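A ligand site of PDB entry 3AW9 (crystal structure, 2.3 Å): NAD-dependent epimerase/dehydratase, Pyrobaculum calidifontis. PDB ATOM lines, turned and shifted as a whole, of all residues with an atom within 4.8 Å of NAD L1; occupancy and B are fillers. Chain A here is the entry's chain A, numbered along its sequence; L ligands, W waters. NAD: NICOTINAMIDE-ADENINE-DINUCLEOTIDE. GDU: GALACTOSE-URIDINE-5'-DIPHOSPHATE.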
ATOM      1  N   GLY A   7      -9.218  -5.664  -0.404  1.00  0.00           N
ATOM      2  CA  GLY A   7      -8.117  -4.757  -0.509  1.00  0.00           C
ATOM      3  C   GLY A   7      -6.956  -5.339  -1.328  1.00  0.00           C
ATOM      4  O   GLY A   7      -5.810  -4.900  -1.184  1.00  0.00           O
ATOM      5  N   ALA A   9      -5.842  -5.032  -4.164  1.00  0.00           N
ATOM      6  CA  ALA A   9      -5.098  -4.182  -5.093  1.00  0.00           C
ATOM      7  C   ALA A   9      -4.056  -3.309  -4.374  1.00  0.00           C
ATOM      8  O   ALA A   9      -3.155  -2.739  -5.006  1.00  0.00           O
ATOM      9  CB  ALA A   9      -6.072  -3.299  -5.898  1.00  0.00           C
ATOM     10  N   GLY A  10      -4.196  -3.212  -3.053  1.00  0.00           N
ATOM     11  CA  GLY A  10      -3.331  -2.366  -2.245  1.00  0.00           C
ATOM     12  C   GLY A  10      -2.005  -2.992  -1.844  1.00  0.00           C
ATOM     13  O   GLY A  10      -1.618  -4.010  -2.385  1.00  0.00           O
ATOM     14  N   PHE A  11      -1.322  -2.368  -0.892  1.00  0.00           N
ATOM     15  CA  PHE A  11       0.060  -2.701  -0.565  1.00  0.00           C
ATOM     16  C   PHE A  11       0.232  -4.144  -0.094  1.00  0.00           C
ATOM     17  O   PHE A  11       0.701  -4.977  -0.883  1.00  0.00           O
ATOM     18  CB  PHE A  11       0.687  -1.671   0.379  1.00  0.00           C
ATOM     19  CG  PHE A  11       2.012  -2.090   0.973  1.00  0.00           C
ATOM     20  CD1 PHE A  11       3.096  -2.440   0.158  1.00  0.00           C
ATOM     21  CD2 PHE A  11       2.167  -2.142   2.365  1.00  0.00           C
ATOM     22  CE1 PHE A  11       4.316  -2.844   0.720  1.00  0.00           C
ATOM     23  CE2 PHE A  11       3.371  -2.532   2.934  1.00  0.00           C
ATOM     24  CZ  PHE A  11       4.453  -2.884   2.104  1.00  0.00           C
ATOM     25  N   ILE A  12      -0.145  -4.435   1.147  1.00  0.00           N
ATOM     26  CA  ILE A  12      -0.029  -5.798   1.692  1.00  0.00           C
ATOM     27  C   ILE A  12      -0.881  -6.820   0.893  1.00  0.00           C
ATOM     28  O   ILE A  12      -0.385  -7.888   0.530  1.00  0.00           O
ATOM     29  CB  ILE A  12      -0.346  -5.892   3.210  1.00  0.00           C
ATOM     30  CG1 ILE A  12       0.465  -4.864   3.989  1.00  0.00           C
ATOM     31  CG2 ILE A  12      -0.079  -7.327   3.733  1.00  0.00           C
ATOM     32  CD1 ILE A  12       0.236  -4.905   5.476  1.00  0.00           C
ATOM     33  N   GLY A  13      -2.133  -6.470   0.607  1.00  0.00           N
ATOM     34  CA  GLY A  13      -3.070  -7.314  -0.141  1.00  0.00           C
ATOM     35  C   GLY A  13      -2.548  -7.862  -1.465  1.00  0.00           C
ATOM     36  O   GLY A  13      -2.605  -9.061  -1.696  1.00  0.00           O
ATOM     37  N   VAL A  30     -10.848  -8.544  -4.294  1.00  0.00           N
ATOM     38  CA  VAL A  30     -11.944  -7.555  -4.178  1.00  0.00           C
ATOM     39  C   VAL A  30     -11.375  -6.230  -3.686  1.00  0.00           C
ATOM     40  O   VAL A  30     -10.786  -6.147  -2.620  1.00  0.00           O
ATOM     41  CB  VAL A  30     -13.135  -8.037  -3.277  1.00  0.00           C
ATOM     42  CG1 VAL A  30     -14.167  -6.920  -3.078  1.00  0.00           C
ATOM     43  CG2 VAL A  30     -13.801  -9.306  -3.841  1.00  0.00           C
ATOM     44  N   ASP A  31     -11.550  -5.175  -4.469  1.00  0.00           N
ATOM     45  CA  ASP A  31     -11.002  -3.891  -4.121  1.00  0.00           C
ATOM     46  C   ASP A  31     -11.816  -2.838  -4.815  1.00  0.00           C
ATOM     47  O   ASP A  31     -12.444  -3.116  -5.838  1.00  0.00           O
ATOM     48  CB  ASP A  31      -9.531  -3.790  -4.544  1.00  0.00           C
ATOM     49  CG  ASP A  31      -8.777  -2.721  -3.794  1.00  0.00           C
ATOM     50  OD1 ASP A  31      -9.089  -1.523  -3.958  1.00  0.00           O
ATOM     51  OD2 ASP A  31      -7.863  -3.080  -3.015  1.00  0.00           O
ATOM     52  N   ILE A  32     -11.813  -1.640  -4.247  1.00  0.00           N
ATOM     53  CA  ILE A  32     -12.542  -0.511  -4.817  1.00  0.00           C
ATOM     54  C   ILE A  32     -11.771   0.116  -5.996  1.00  0.00           C
ATOM     55  O   ILE A  32     -12.340   0.871  -6.766  1.00  0.00           O
ATOM     56  CB  ILE A  32     -12.920   0.538  -3.712  1.00  0.00           C
ATOM     57  CG1 ILE A  32     -14.197   1.306  -4.107  1.00  0.00           C
ATOM     58  CG2 ILE A  32     -11.725   1.430  -3.358  1.00  0.00           C
ATOM     59  CD1 ILE A  32     -14.749   2.303  -3.080  1.00  0.00           C
ATOM     60  N   VAL A  33     -10.487  -0.198  -6.121  1.00  0.00           N
ATOM     61  CA  VAL A  33      -9.691   0.257  -7.271  1.00  0.00           C
ATOM     62  C   VAL A  33      -9.277  -0.941  -8.122  1.00  0.00           C
ATOM     63  O   VAL A  33      -9.225  -2.080  -7.645  1.00  0.00           O
ATOM     64  CB  VAL A  33      -8.415   1.128  -6.883  1.00  0.00           C
ATOM     65  CG1 VAL A  33      -8.777   2.257  -5.942  1.00  0.00           C
ATOM     66  CG2 VAL A  33      -7.308   0.279  -6.280  1.00  0.00           C
ATOM     67  N   ARG A  46     -15.561  -3.652  -6.026  1.00  0.00           N
ATOM     68  CA  ARG A  46     -16.693  -3.493  -5.104  1.00  0.00           C
ATOM     69  C   ARG A  46     -16.322  -2.495  -4.009  1.00  0.00           C
ATOM     70  O   ARG A  46     -15.145  -2.316  -3.692  1.00  0.00           O
ATOM     71  CB  ARG A  46     -17.066  -4.816  -4.404  1.00  0.00           C
ATOM     72  CG  ARG A  46     -17.325  -6.018  -5.293  1.00  0.00           C
ATOM     73  CD  ARG A  46     -18.618  -5.872  -6.083  1.00  0.00           C
ATOM     74  NE  ARG A  46     -18.709  -6.881  -7.120  1.00  0.00           N
ATOM     75  CZ  ARG A  46     -19.526  -7.932  -7.057  1.00  0.00           C
ATOM     76  NH1 ARG A  46     -20.336  -8.081  -6.015  1.00  0.00           N
ATOM     77  NH2 ARG A  46     -19.544  -8.826  -8.052  1.00  0.00           N
ATOM     78  N   ASP A  47     -17.340  -1.867  -3.422  1.00  0.00           N
ATOM     79  CA  ASP A  47     -17.190  -1.028  -2.243  1.00  0.00           C
ATOM     80  C   ASP A  47     -17.772  -1.791  -1.040  1.00  0.00           C
ATOM     81  O   ASP A  47     -18.969  -2.004  -0.968  1.00  0.00           O
ATOM     82  CB  ASP A  47     -17.932   0.277  -2.460  1.00  0.00           C
ATOM     83  CG  ASP A  47     -17.819   1.261  -1.287  1.00  0.00           C
ATOM     84  OD1 ASP A  47     -17.049   1.059  -0.296  1.00  0.00           O
ATOM     85  OD2 ASP A  47     -18.535   2.288  -1.393  1.00  0.00           O
ATOM     86  N   LEU A  48     -16.896  -2.204  -0.118  1.00  0.00           N
ATOM     87  CA  LEU A  48     -17.270  -2.909   1.127  1.00  0.00           C
ATOM     88  C   LEU A  48     -18.132  -2.129   2.140  1.00  0.00           C
ATOM     89  O   LEU A  48     -18.722  -2.732   3.044  1.00  0.00           O
ATOM     90  CB  LEU A  48     -16.008  -3.462   1.787  1.00  0.00           C
ATOM     91  CG  LEU A  48     -15.538  -4.858   1.329  1.00  0.00           C
ATOM     92  CD1 LEU A  48     -15.299  -4.907  -0.186  1.00  0.00           C
ATOM     93  CD2 LEU A  48     -14.305  -5.262   2.061  1.00  0.00           C
ATOM     94  N   LYS A  49     -18.271  -0.817   1.950  1.00  0.00           N
ATOM     95  CA  LYS A  49     -19.241  -0.032   2.733  1.00  0.00           C
ATOM     96  C   LYS A  49     -20.667  -0.401   2.297  1.00  0.00           C
ATOM     97  O   LYS A  49     -21.637  -0.115   3.028  1.00  0.00           O
ATOM     98  CB  LYS A  49     -19.011   1.483   2.612  1.00  0.00           C
ATOM     99  CG  LYS A  49     -17.623   1.975   3.058  1.00  0.00           C
ATOM    100  CD  LYS A  49     -17.479   3.522   3.038  1.00  0.00           C
ATOM    101  CE  LYS A  49     -17.345   4.114   1.624  1.00  0.00           C
ATOM    102  NZ  LYS A  49     -16.194   3.501   0.894  1.00  0.00           N
ATOM    103  N   PHE A  65      -8.404  -7.113   4.133  1.00  0.00           N
ATOM    104  CA  PHE A  65      -7.306  -6.150   4.144  1.00  0.00           C
ATOM    105  C   PHE A  65      -7.769  -4.837   3.550  1.00  0.00           C
ATOM    106  O   PHE A  65      -6.971  -3.927   3.388  1.00  0.00           O
ATOM    107  CB  PHE A  65      -6.053  -6.715   3.425  1.00  0.00           C
ATOM    108  CG  PHE A  65      -5.241  -7.651   4.293  1.00  0.00           C
ATOM    109  CD1 PHE A  65      -5.800  -8.841   4.769  1.00  0.00           C
ATOM    110  CD2 PHE A  65      -3.946  -7.312   4.681  1.00  0.00           C
ATOM    111  CE1 PHE A  65      -5.072  -9.701   5.605  1.00  0.00           C
ATOM    112  CE2 PHE A  65      -3.217  -8.148   5.515  1.00  0.00           C
ATOM    113  CZ  PHE A  65      -3.778  -9.363   5.979  1.00  0.00           C
ATOM    114  N   ALA A  66      -9.057  -4.737   3.205  1.00  0.00           N
ATOM    115  CA  ALA A  66      -9.649  -3.466   2.778  1.00  0.00           C
ATOM    116  C   ALA A  66      -9.858  -2.566   3.989  1.00  0.00           C
ATOM    117  O   ALA A  66     -10.478  -2.954   4.974  1.00  0.00           O
ATOM    118  CB  ALA A  66     -10.968  -3.701   2.061  1.00  0.00           C
ATOM    119  N   ALA A  67      -9.316  -1.361   3.911  1.00  0.00           N
ATOM    120  CA  ALA A  67      -9.404  -0.370   4.987  1.00  0.00           C
ATOM    121  C   ALA A  67      -8.860   0.958   4.484  1.00  0.00           C
ATOM    122  O   ALA A  67      -8.298   1.044   3.403  1.00  0.00           O
ATOM    123  CB  ALA A  67      -8.598  -0.837   6.229  1.00  0.00           C
ATOM    124  N   PRO A  69      -5.974   3.133   5.770  1.00  0.00           N
ATOM    125  CA  PRO A  69      -4.874   2.932   6.731  1.00  0.00           C
ATOM    126  C   PRO A  69      -4.379   4.186   7.497  1.00  0.00           C
ATOM    127  O   PRO A  69      -3.623   4.044   8.463  1.00  0.00           O
ATOM    128  CB  PRO A  69      -3.773   2.354   5.865  1.00  0.00           C
ATOM    129  CG  PRO A  69      -4.017   2.996   4.479  1.00  0.00           C
ATOM    130  CD  PRO A  69      -5.495   3.229   4.372  1.00  0.00           C
ATOM    131  N   GLU A  84     -15.306   3.001   6.687  1.00  0.00           N
ATOM    132  CA  GLU A  84     -14.234   2.290   5.999  1.00  0.00           C
ATOM    133  C   GLU A  84     -13.681   1.143   6.829  1.00  0.00           C
ATOM    134  O   GLU A  84     -13.337   0.096   6.293  1.00  0.00           O
ATOM    135  CB  GLU A  84     -13.091   3.264   5.686  1.00  0.00           C
ATOM    136  CG  GLU A  84     -13.305   4.028   4.435  1.00  0.00           C
ATOM    137  CD  GLU A  84     -13.172   3.111   3.223  1.00  0.00           C
ATOM    138  OE1 GLU A  84     -12.034   2.622   2.944  1.00  0.00           O
ATOM    139  OE2 GLU A  84     -14.209   2.903   2.568  1.00  0.00           O
ATOM    140  N   ALA A 107      -6.725  -8.153   8.930  1.00  0.00           N
ATOM    141  CA  ALA A 107      -5.641  -7.178   9.139  1.00  0.00           C
ATOM    142  C   ALA A 107      -5.978  -6.235  10.282  1.00  0.00           C
ATOM    143  O   ALA A 107      -6.806  -5.328  10.150  1.00  0.00           O
ATOM    144  CB  ALA A 107      -5.372  -6.389   7.884  1.00  0.00           C
ATOM    145  N   SER A 108      -5.341  -6.453  11.416  1.00  0.00           N
ATOM    146  CA  SER A 108      -5.439  -5.563  12.545  1.00  0.00           C
ATOM    147  C   SER A 108      -4.123  -4.746  12.580  1.00  0.00           C
ATOM    148  O   SER A 108      -3.466  -4.563  11.542  1.00  0.00           O
ATOM    149  CB  SER A 108      -5.649  -6.369  13.827  1.00  0.00           C
ATOM    150  OG  SER A 108      -6.007  -5.511  14.886  1.00  0.00           O
ATOM    151  N   SER A 109      -3.741  -4.274  13.753  1.00  0.00           N
ATOM    152  CA  SER A 109      -2.727  -3.243  13.868  1.00  0.00           C
ATOM    153  C   SER A 109      -2.284  -3.070  15.295  1.00  0.00           C
ATOM    154  O   SER A 109      -3.069  -3.282  16.214  1.00  0.00           O
ATOM    155  CB  SER A 109      -3.271  -1.893  13.346  1.00  0.00           C
ATOM    156  OG  SER A 109      -2.492  -0.770  13.783  1.00  0.00           O
ATOM    157  N   TYR A 133      -8.857   5.175  14.392  1.00  0.00           N
ATOM    158  CA  TYR A 133      -8.366   4.031  13.631  1.00  0.00           C
ATOM    159  C   TYR A 133      -8.036   2.800  14.515  1.00  0.00           C
ATOM    160  O   TYR A 133      -8.411   1.664  14.188  1.00  0.00           O
ATOM    161  CB  TYR A 133      -7.145   4.473  12.811  1.00  0.00           C
ATOM    162  CG  TYR A 133      -6.412   3.361  12.106  1.00  0.00           C
ATOM    163  CD1 TYR A 133      -6.880   2.836  10.878  1.00  0.00           C
ATOM    164  CD2 TYR A 133      -5.248   2.819  12.642  1.00  0.00           C
ATOM    165  CE1 TYR A 133      -6.175   1.804  10.210  1.00  0.00           C
ATOM    166  CE2 TYR A 133      -4.553   1.809  11.994  1.00  0.00           C
ATOM    167  CZ  TYR A 133      -5.012   1.308  10.798  1.00  0.00           C
ATOM    168  OH  TYR A 133      -4.273   0.309  10.204  1.00  0.00           O
ATOM    169  N   LYS A 137      -9.989  -0.779  14.506  1.00  0.00           N
ATOM    170  CA  LYS A 137      -9.364  -2.116  14.454  1.00  0.00           C
ATOM    171  C   LYS A 137      -9.727  -2.989  15.672  1.00  0.00           C
ATOM    172  O   LYS A 137     -10.006  -4.168  15.508  1.00  0.00           O
ATOM    173  CB  LYS A 137      -7.850  -2.020  14.257  1.00  0.00           C
ATOM    174  CG  LYS A 137      -7.434  -1.402  12.905  1.00  0.00           C
ATOM    175  CD  LYS A 137      -7.869  -2.280  11.744  1.00  0.00           C
ATOM    176  CE  LYS A 137      -7.224  -1.836  10.461  1.00  0.00           C
ATOM    177  NZ  LYS A 137      -7.654  -2.738   9.353  1.00  0.00           N
ATOM    178  N   TYR A 160      -0.460  -6.150  12.841  1.00  0.00           N
ATOM    179  CA  TYR A 160       0.729  -5.651  12.159  1.00  0.00           C
ATOM    180  C   TYR A 160       1.306  -4.378  12.784  1.00  0.00           C
ATOM    181  O   TYR A 160       0.579  -3.401  13.010  1.00  0.00           O
ATOM    182  CB  TYR A 160       0.432  -5.338  10.700  1.00  0.00           C
ATOM    183  CG  TYR A 160       0.049  -6.512   9.857  1.00  0.00           C
ATOM    184  CD1 TYR A 160      -1.289  -6.789   9.579  1.00  0.00           C
ATOM    185  CD2 TYR A 160       1.026  -7.359   9.314  1.00  0.00           C
ATOM    186  CE1 TYR A 160      -1.646  -7.850   8.774  1.00  0.00           C
ATOM    187  CE2 TYR A 160       0.681  -8.428   8.523  1.00  0.00           C
ATOM    188  CZ  TYR A 160      -0.654  -8.666   8.263  1.00  0.00           C
ATOM    189  OH  TYR A 160      -1.011  -9.737   7.480  1.00  0.00           O
ATOM    190  N   ALA A 161       2.623  -4.402  13.007  1.00  0.00           N
ATOM    191  CA  ALA A 161       3.415  -3.203  13.223  1.00  0.00           C
ATOM    192  C   ALA A 161       3.608  -2.592  11.825  1.00  0.00           C
ATOM    193  O   ALA A 161       2.864  -2.942  10.913  1.00  0.00           O
ATOM    194  CB  ALA A 161       4.746  -3.566  13.882  1.00  0.00           C
ATOM    195  N   ASN A 162       4.559  -1.697  11.600  1.00  0.00           N
ATOM    196  CA  ASN A 162       4.642  -1.131  10.269  1.00  0.00           C
ATOM    197  C   ASN A 162       5.184  -2.151   9.294  1.00  0.00           C
ATOM    198  O   ASN A 162       6.118  -2.875   9.603  1.00  0.00           O
ATOM    199  CB  ASN A 162       5.502   0.122  10.235  1.00  0.00           C
ATOM    200  CG  ASN A 162       4.984   1.192  11.146  1.00  0.00           C
ATOM    201  OD1 ASN A 162       4.101   1.954  10.760  1.00  0.00           O
ATOM    202  ND2 ASN A 162       5.509   1.256  12.366  1.00  0.00           N
ATOM    203  N   VAL A 163       4.573  -2.219   8.115  1.00  0.00           N
ATOM    204  CA  VAL A 163       5.033  -3.117   7.076  1.00  0.00           C
ATOM    205  C   VAL A 163       5.429  -2.223   5.925  1.00  0.00           C
ATOM    206  O   VAL A 163       4.702  -1.310   5.575  1.00  0.00           O
ATOM    207  CB  VAL A 163       3.945  -4.117   6.663  1.00  0.00           C
ATOM    208  CG1 VAL A 163       4.420  -4.955   5.490  1.00  0.00           C
ATOM    209  CG2 VAL A 163       3.574  -4.990   7.832  1.00  0.00           C
ATOM    210  N   LEU A 168       4.141   0.456  -1.508  1.00  0.00           N
ATOM    211  CA  LEU A 168       3.654   1.234  -0.371  1.00  0.00           C
ATOM    212  C   LEU A 168       3.445   2.689  -0.792  1.00  0.00           C
ATOM    213  O   LEU A 168       4.305   3.275  -1.452  1.00  0.00           O
ATOM    214  CB  LEU A 168       4.630   1.124   0.808  1.00  0.00           C
ATOM    215  CG  LEU A 168       4.253   1.775   2.136  1.00  0.00           C
ATOM    216  CD1 LEU A 168       2.870   1.357   2.642  1.00  0.00           C
ATOM    217  CD2 LEU A 168       5.300   1.432   3.163  1.00  0.00           C
ATOM    218  N   HIS A 170       1.697   5.012   1.581  1.00  0.00           N
ATOM    219  CA  HIS A 170       1.332   5.774   2.749  1.00  0.00           C
ATOM    220  C   HIS A 170       2.440   5.575   3.774  1.00  0.00           C
ATOM    221  O   HIS A 170       3.281   4.696   3.618  1.00  0.00           O
ATOM    222  CB  HIS A 170      -0.055   5.352   3.298  1.00  0.00           C
ATOM    223  CG  HIS A 170      -0.100   3.946   3.812  1.00  0.00           C
ATOM    224  ND1 HIS A 170       0.118   3.642   5.146  1.00  0.00           N
ATOM    225  CD2 HIS A 170      -0.329   2.768   3.189  1.00  0.00           C
ATOM    226  CE1 HIS A 170       0.053   2.334   5.310  1.00  0.00           C
ATOM    227  NE2 HIS A 170      -0.218   1.775   4.140  1.00  0.00           N
HETATM  228  PA  NAD L   1      -3.456   0.097   1.187  1.00  0.00           P
HETATM  229  O1A NAD L   1      -2.315  -0.073   0.238  1.00  0.00           O
HETATM  230  O2A NAD L   1      -4.241   1.345   1.156  1.00  0.00           O
HETATM  231  O5B NAD L   1      -4.478  -1.141   0.930  1.00  0.00           O
HETATM  232  C5B NAD L   1      -5.865  -1.097   1.206  1.00  0.00           C
HETATM  233  C4B NAD L   1      -6.686  -1.429  -0.023  1.00  0.00           C
HETATM  234  O4B NAD L   1      -8.088  -1.387   0.433  1.00  0.00           O
HETATM  235  C3B NAD L   1      -6.550  -0.324  -1.074  1.00  0.00           C
HETATM  236  O3B NAD L   1      -6.184  -0.907  -2.345  1.00  0.00           O
HETATM  237  C2B NAD L   1      -7.959   0.305  -1.087  1.00  0.00           C
HETATM  238  O2B NAD L   1      -8.379   0.674  -2.389  1.00  0.00           O
HETATM  239  C1B NAD L   1      -8.860  -0.814  -0.602  1.00  0.00           C
HETATM  240  N9A NAD L   1     -10.188  -0.292  -0.068  1.00  0.00           N
HETATM  241  C8A NAD L   1     -10.352   0.732   0.795  1.00  0.00           C
HETATM  242  N7A NAD L   1     -11.645   0.915   1.040  1.00  0.00           N
HETATM  243  C5A NAD L   1     -12.317  -0.003   0.371  1.00  0.00           C
HETATM  244  C6A NAD L   1     -13.673  -0.309   0.247  1.00  0.00           C
HETATM  245  N6A NAD L   1     -14.585   0.397   0.899  1.00  0.00           N
HETATM  246  N1A NAD L   1     -14.044  -1.320  -0.563  1.00  0.00           N
HETATM  247  C2A NAD L   1     -13.139  -2.023  -1.222  1.00  0.00           C
HETATM  248  N3A NAD L   1     -11.844  -1.761  -1.126  1.00  0.00           N
HETATM  249  C4A NAD L   1     -11.400  -0.774  -0.346  1.00  0.00           C
HETATM  250  O3  NAD L   1      -3.002  -0.165   2.712  1.00  0.00           O
HETATM  251  PN  NAD L   1      -2.033  -1.301   3.236  1.00  0.00           P
HETATM  252  O1N NAD L   1      -0.859  -0.629   3.840  1.00  0.00           O
HETATM  253  O2N NAD L   1      -1.881  -2.302   2.187  1.00  0.00           O
HETATM  254  O5D NAD L   1      -2.779  -2.008   4.450  1.00  0.00           O
HETATM  255  C5D NAD L   1      -3.902  -2.909   4.186  1.00  0.00           C
HETATM  256  C4D NAD L   1      -4.453  -3.529   5.481  1.00  0.00           C
HETATM  257  O4D NAD L   1      -3.340  -3.760   6.388  1.00  0.00           O
HETATM  258  C3D NAD L   1      -5.365  -2.483   6.158  1.00  0.00           C
HETATM  259  O3D NAD L   1      -6.393  -3.139   6.933  1.00  0.00           O
HETATM  260  C2D NAD L   1      -4.385  -1.794   7.068  1.00  0.00           C
HETATM  261  O2D NAD L   1      -5.093  -1.037   8.069  1.00  0.00           O
HETATM  262  C1D NAD L   1      -3.636  -3.035   7.606  1.00  0.00           C
HETATM  263  N1N NAD L   1      -2.333  -2.711   8.215  1.00  0.00           N
HETATM  264  C2N NAD L   1      -1.256  -2.266   7.416  1.00  0.00           C
HETATM  265  C3N NAD L   1      -0.035  -1.955   8.016  1.00  0.00           C
HETATM  266  C7N NAD L   1       1.143  -1.453   7.192  1.00  0.00           C
HETATM  267  O7N NAD L   1       2.183  -1.142   7.759  1.00  0.00           O
HETATM  268  N7N NAD L   1       0.949  -1.345   5.875  1.00  0.00           N
HETATM  269  C4N NAD L   1       0.111  -2.041   9.397  1.00  0.00           C
HETATM  270  C5N NAD L   1      -0.970  -2.457  10.187  1.00  0.00           C
HETATM  271  C6N NAD L   1      -2.186  -2.797   9.596  1.00  0.00           C
HETATM  272  N1  GDU L   2       5.822  11.100  11.108  1.00  0.00           N
HETATM  273  C2  GDU L   2       6.422  12.312  10.763  1.00  0.00           C
HETATM  274  N3  GDU L   2       6.169  12.902   9.510  1.00  0.00           N
HETATM  275  C4  GDU L   2       5.280  12.270   8.611  1.00  0.00           C
HETATM  276  C5  GDU L   2       4.656  11.063   8.949  1.00  0.00           C
HETATM  277  C6  GDU L   2       4.926  10.470  10.188  1.00  0.00           C
HETATM  278  O2  GDU L   2       7.196  12.841  11.549  1.00  0.00           O
HETATM  279  O4  GDU L   2       5.064  12.811   7.510  1.00  0.00           O
HETATM  280  C1D GDU L   2       6.135  10.554  12.475  1.00  0.00           C
HETATM  281  C2D GDU L   2       4.833  10.224  13.253  1.00  0.00           C
HETATM  282  O2D GDU L   2       4.660  11.165  14.316  1.00  0.00           O
HETATM  283  C3D GDU L   2       5.026   8.799  13.800  1.00  0.00           C
HETATM  284  C4D GDU L   2       6.251   8.255  13.059  1.00  0.00           C
HETATM  285  O4D GDU L   2       6.974   9.362  12.477  1.00  0.00           O
HETATM  286  O3D GDU L   2       5.295   8.811  15.201  1.00  0.00           O
HETATM  287  C5D GDU L   2       5.746   7.327  11.971  1.00  0.00           C
HETATM  288  O5D GDU L   2       5.448   6.072  12.575  1.00  0.00           O
HETATM  289  PA  GDU L   2       4.792   4.874  11.734  1.00  0.00           P
HETATM  290  O1A GDU L   2       4.168   3.971  12.704  1.00  0.00           O
HETATM  291  O2A GDU L   2       5.790   4.355  10.789  1.00  0.00           O
HETATM  292  O3A GDU L   2       3.708   5.660  10.801  1.00  0.00           O
HETATM  293  PB  GDU L   2       2.214   5.883  11.287  1.00  0.00           P
HETATM  294  O1B GDU L   2       1.580   6.718  10.249  1.00  0.00           O
HETATM  295  O2B GDU L   2       2.251   6.340  12.692  1.00  0.00           O
HETATM  296  O3B GDU L   2       1.648   4.327  11.214  1.00  0.00           O
HETATM  297  C1' GDU L   2       0.549   3.740  11.972  1.00  0.00           C
HETATM  298  C2' GDU L   2       0.897   2.461  12.803  1.00  0.00           C
HETATM  299  C3' GDU L   2       1.011   1.150  11.998  1.00  0.00           C
HETATM  300  C4' GDU L   2       0.033   1.043  10.819  1.00  0.00           C
HETATM  301  C5' GDU L   2      -0.064   2.389  10.083  1.00  0.00           C
HETATM  302  C6' GDU L   2      -0.972   2.322   8.854  1.00  0.00           C
HETATM  303  O2' GDU L   2       2.131   2.635  13.515  1.00  0.00           O
HETATM  304  O3' GDU L   2       0.803   0.029  12.877  1.00  0.00           O
HETATM  305  O4' GDU L   2      -1.255   0.606  11.279  1.00  0.00           O
HETATM  306  O5' GDU L   2      -0.508   3.405  11.031  1.00  0.00           O
HETATM  307  O6' GDU L   2      -0.937   3.586   8.190  1.00  0.00           O
HETATM  308  O   HOH W   1      -0.407   2.022   0.164  1.00  0.00           O
HETATM  309  O   HOH W   2      -8.872  -4.618   6.819  1.00  0.00           O
HETATM  310  O   HOH W   3      -2.161   0.932  -2.398  1.00  0.00           O
HETATM  311  O   HOH W   4      -6.570   2.420   1.153  1.00  0.00           O
HETATM  312  O   HOH W   5      -3.847  -4.348   0.843  1.00  0.00           O
HETATM  313  O   HOH W   6      -4.679   0.774  -3.767  1.00  0.00           O
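The backbone carbonyl oxygen (O) of Arg 46 lies close to a nitrogen (N1A) of NAD L1 (3.5 Å). A nitrogen (N6A) of NAD L1 sits close to the side-chain amino group (NZ) of Lys 49 (3.5 Å). Gly 7 touches NAD L1 (CA to O4B, 3.5 Å). Ala 9 touches NAD L1 (C to O3B, 3.8 Å). Val 33 touches NAD L1 (CG1 to O2B, 3.9 Å). Phe 65 touches NAD L1. Ala 66 touches NAD L1. Ala 67 touches NAD L1. Pro 69 touches NAD L1 (CG to O2A, 3.7 Å). Ala 107 touches NAD L1. Ser 108 touches NAD L1 (O to C6N, 2.9 Å). Ser 109 touches NAD L1. Tyr 160 touches NAD L1. Ala 161 touches NAD L1. Asn 162 touches NAD L1 (CA to O7N, 3.5 Å). Hydrophobic or aromatic side chains that line NAD L1: Phe 11, Ile 12, Ile 32, Val 33, Leu 48, Phe 65, Ala 66, Ala 67, Pro 69, Ala 107, Tyr 133, Tyr 160, Val 163 and His 170. Within 4 Å of NAD L1: Gly 7, Ala 9, Gly 10, Phe 11, Ile 12, Asp 31, Ile 32, Val 33, Arg 46, Asp 47, Leu 48, Lys 49, Phe 65, Ala 66, Ala 67, Pro 69, Glu 84, Ala 107, Ser 108, Ser 109, Tyr 133, Lys 137, Tyr 160, Ala 161, Asn 162, Val 163 and His 170.
Water W4 bridges an oxygen (O2A) of NAD L1 (2.6 Å) and the backbone carbonyl oxygen of Ala 67 (3.2 Å). Water W2 lies within hydrogen-bond range of O3D of NAD L1, O of Ala 66 and NZ of Lys 137. Water W5 lies within hydrogen-bond range of N of Gly 13 (2.7 Å), O of Gly 7 (2.9 Å) and O2N of NAD L1 (3.1 Å).
NE2 of His 170 is in hydrogen-bond range of O1N of NAD L1 (2.5 Å). The side-chain carboxylate of Glu 84 is in hydrogen-bond range of a nitrogen (N7A) of NAD L1, 2.6 Å away. The backbone NH (N) of Val 163 sits at hydrogen-bond distance from an oxygen (O7N) of NAD L1 (2.6 Å). The side-chain hydroxyl (OH) of Tyr 133 sits at hydrogen-bond distance from an oxygen (O2D) of NAD L1, at 2.7 Å. N of Phe 11 lies within hydrogen-bond range of O1A of NAD L1 (2.7 Å). NZ of Lys 137 is in hydrogen-bond range of O3D of NAD L1 (2.8 Å). The side-chain carboxylate of Asp 31 lies within hydrogen-bond range of an oxygen (O2B) of NAD L1. The side-chain carboxylate (OD1) of Asp 47 is in hydrogen-bond range of a nitrogen (N6A) of NAD L1, at 2.8 Å. The backbone NH (N) of Ile 12 sits at hydrogen-bond distance from an oxygen (O2N) of NAD L1 (2.9 Å). N1A of NAD L1 is in hydrogen-bond range of N of Leu 48 (3.0 Å). The backbone NH of Ile 32 lies within hydrogen-bond range of a nitrogen (N3A) of NAD L1 (3.1 Å). N of Gly 10 is in hydrogen-bond range of O3B of NAD L1. O6' of GDU L2 sits at hydrogen-bond distance from ND1 of His 170. The side-chain hydroxyl of Tyr 133 is in hydrogen-bond range of an oxygen (O4') of GDU L2, at 3.2 Å. O of Tyr 160 is in hydrogen-bond range of O3' of GDU L2 (3.4 Å). An oxygen (O1A) of GDU L2 lies close to the side-chain amide oxygen of Asn 162, 2.8 Å away. The backbone carbonyl oxygen (O) of Pro 69 is in hydrogen-bond range of an oxygen (O6') of GDU L2 (2.7 Å). OG of Ser 109 is in hydrogen-bond range of O4' of GDU L2.
OE2 of Glu 84 lies within salt-bridge range of NZ of Lys 49, at 2.7 Å. NZ of Lys 137 is in hydrogen-bond range of O of Ala 107, at 2.8 Å. O of Asp 31 is in hydrogen-bond range of N of Arg 46, at 3.2 Å. OD2 of Asp 31 sits at hydrogen-bond distance from N of Ala 9, at 3.0 Å. N of Val 33 sits at hydrogen-bond distance from OD1 of Asp 31. The side-chain amino group (NZ) of Lys 49 lies within salt-bridge range of the side-chain carboxylate (OD1) of Asp 47 (2.8 Å). The backbone carbonyl oxygen (O) of Arg 46 sits close to the backbone NH (N) of Ile 32 (3.4 Å). The backbone NH (N) of Gly 7 lies within hydrogen-bond range of the backbone carbonyl oxygen (O) of Val 30, 2.8 Å away.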
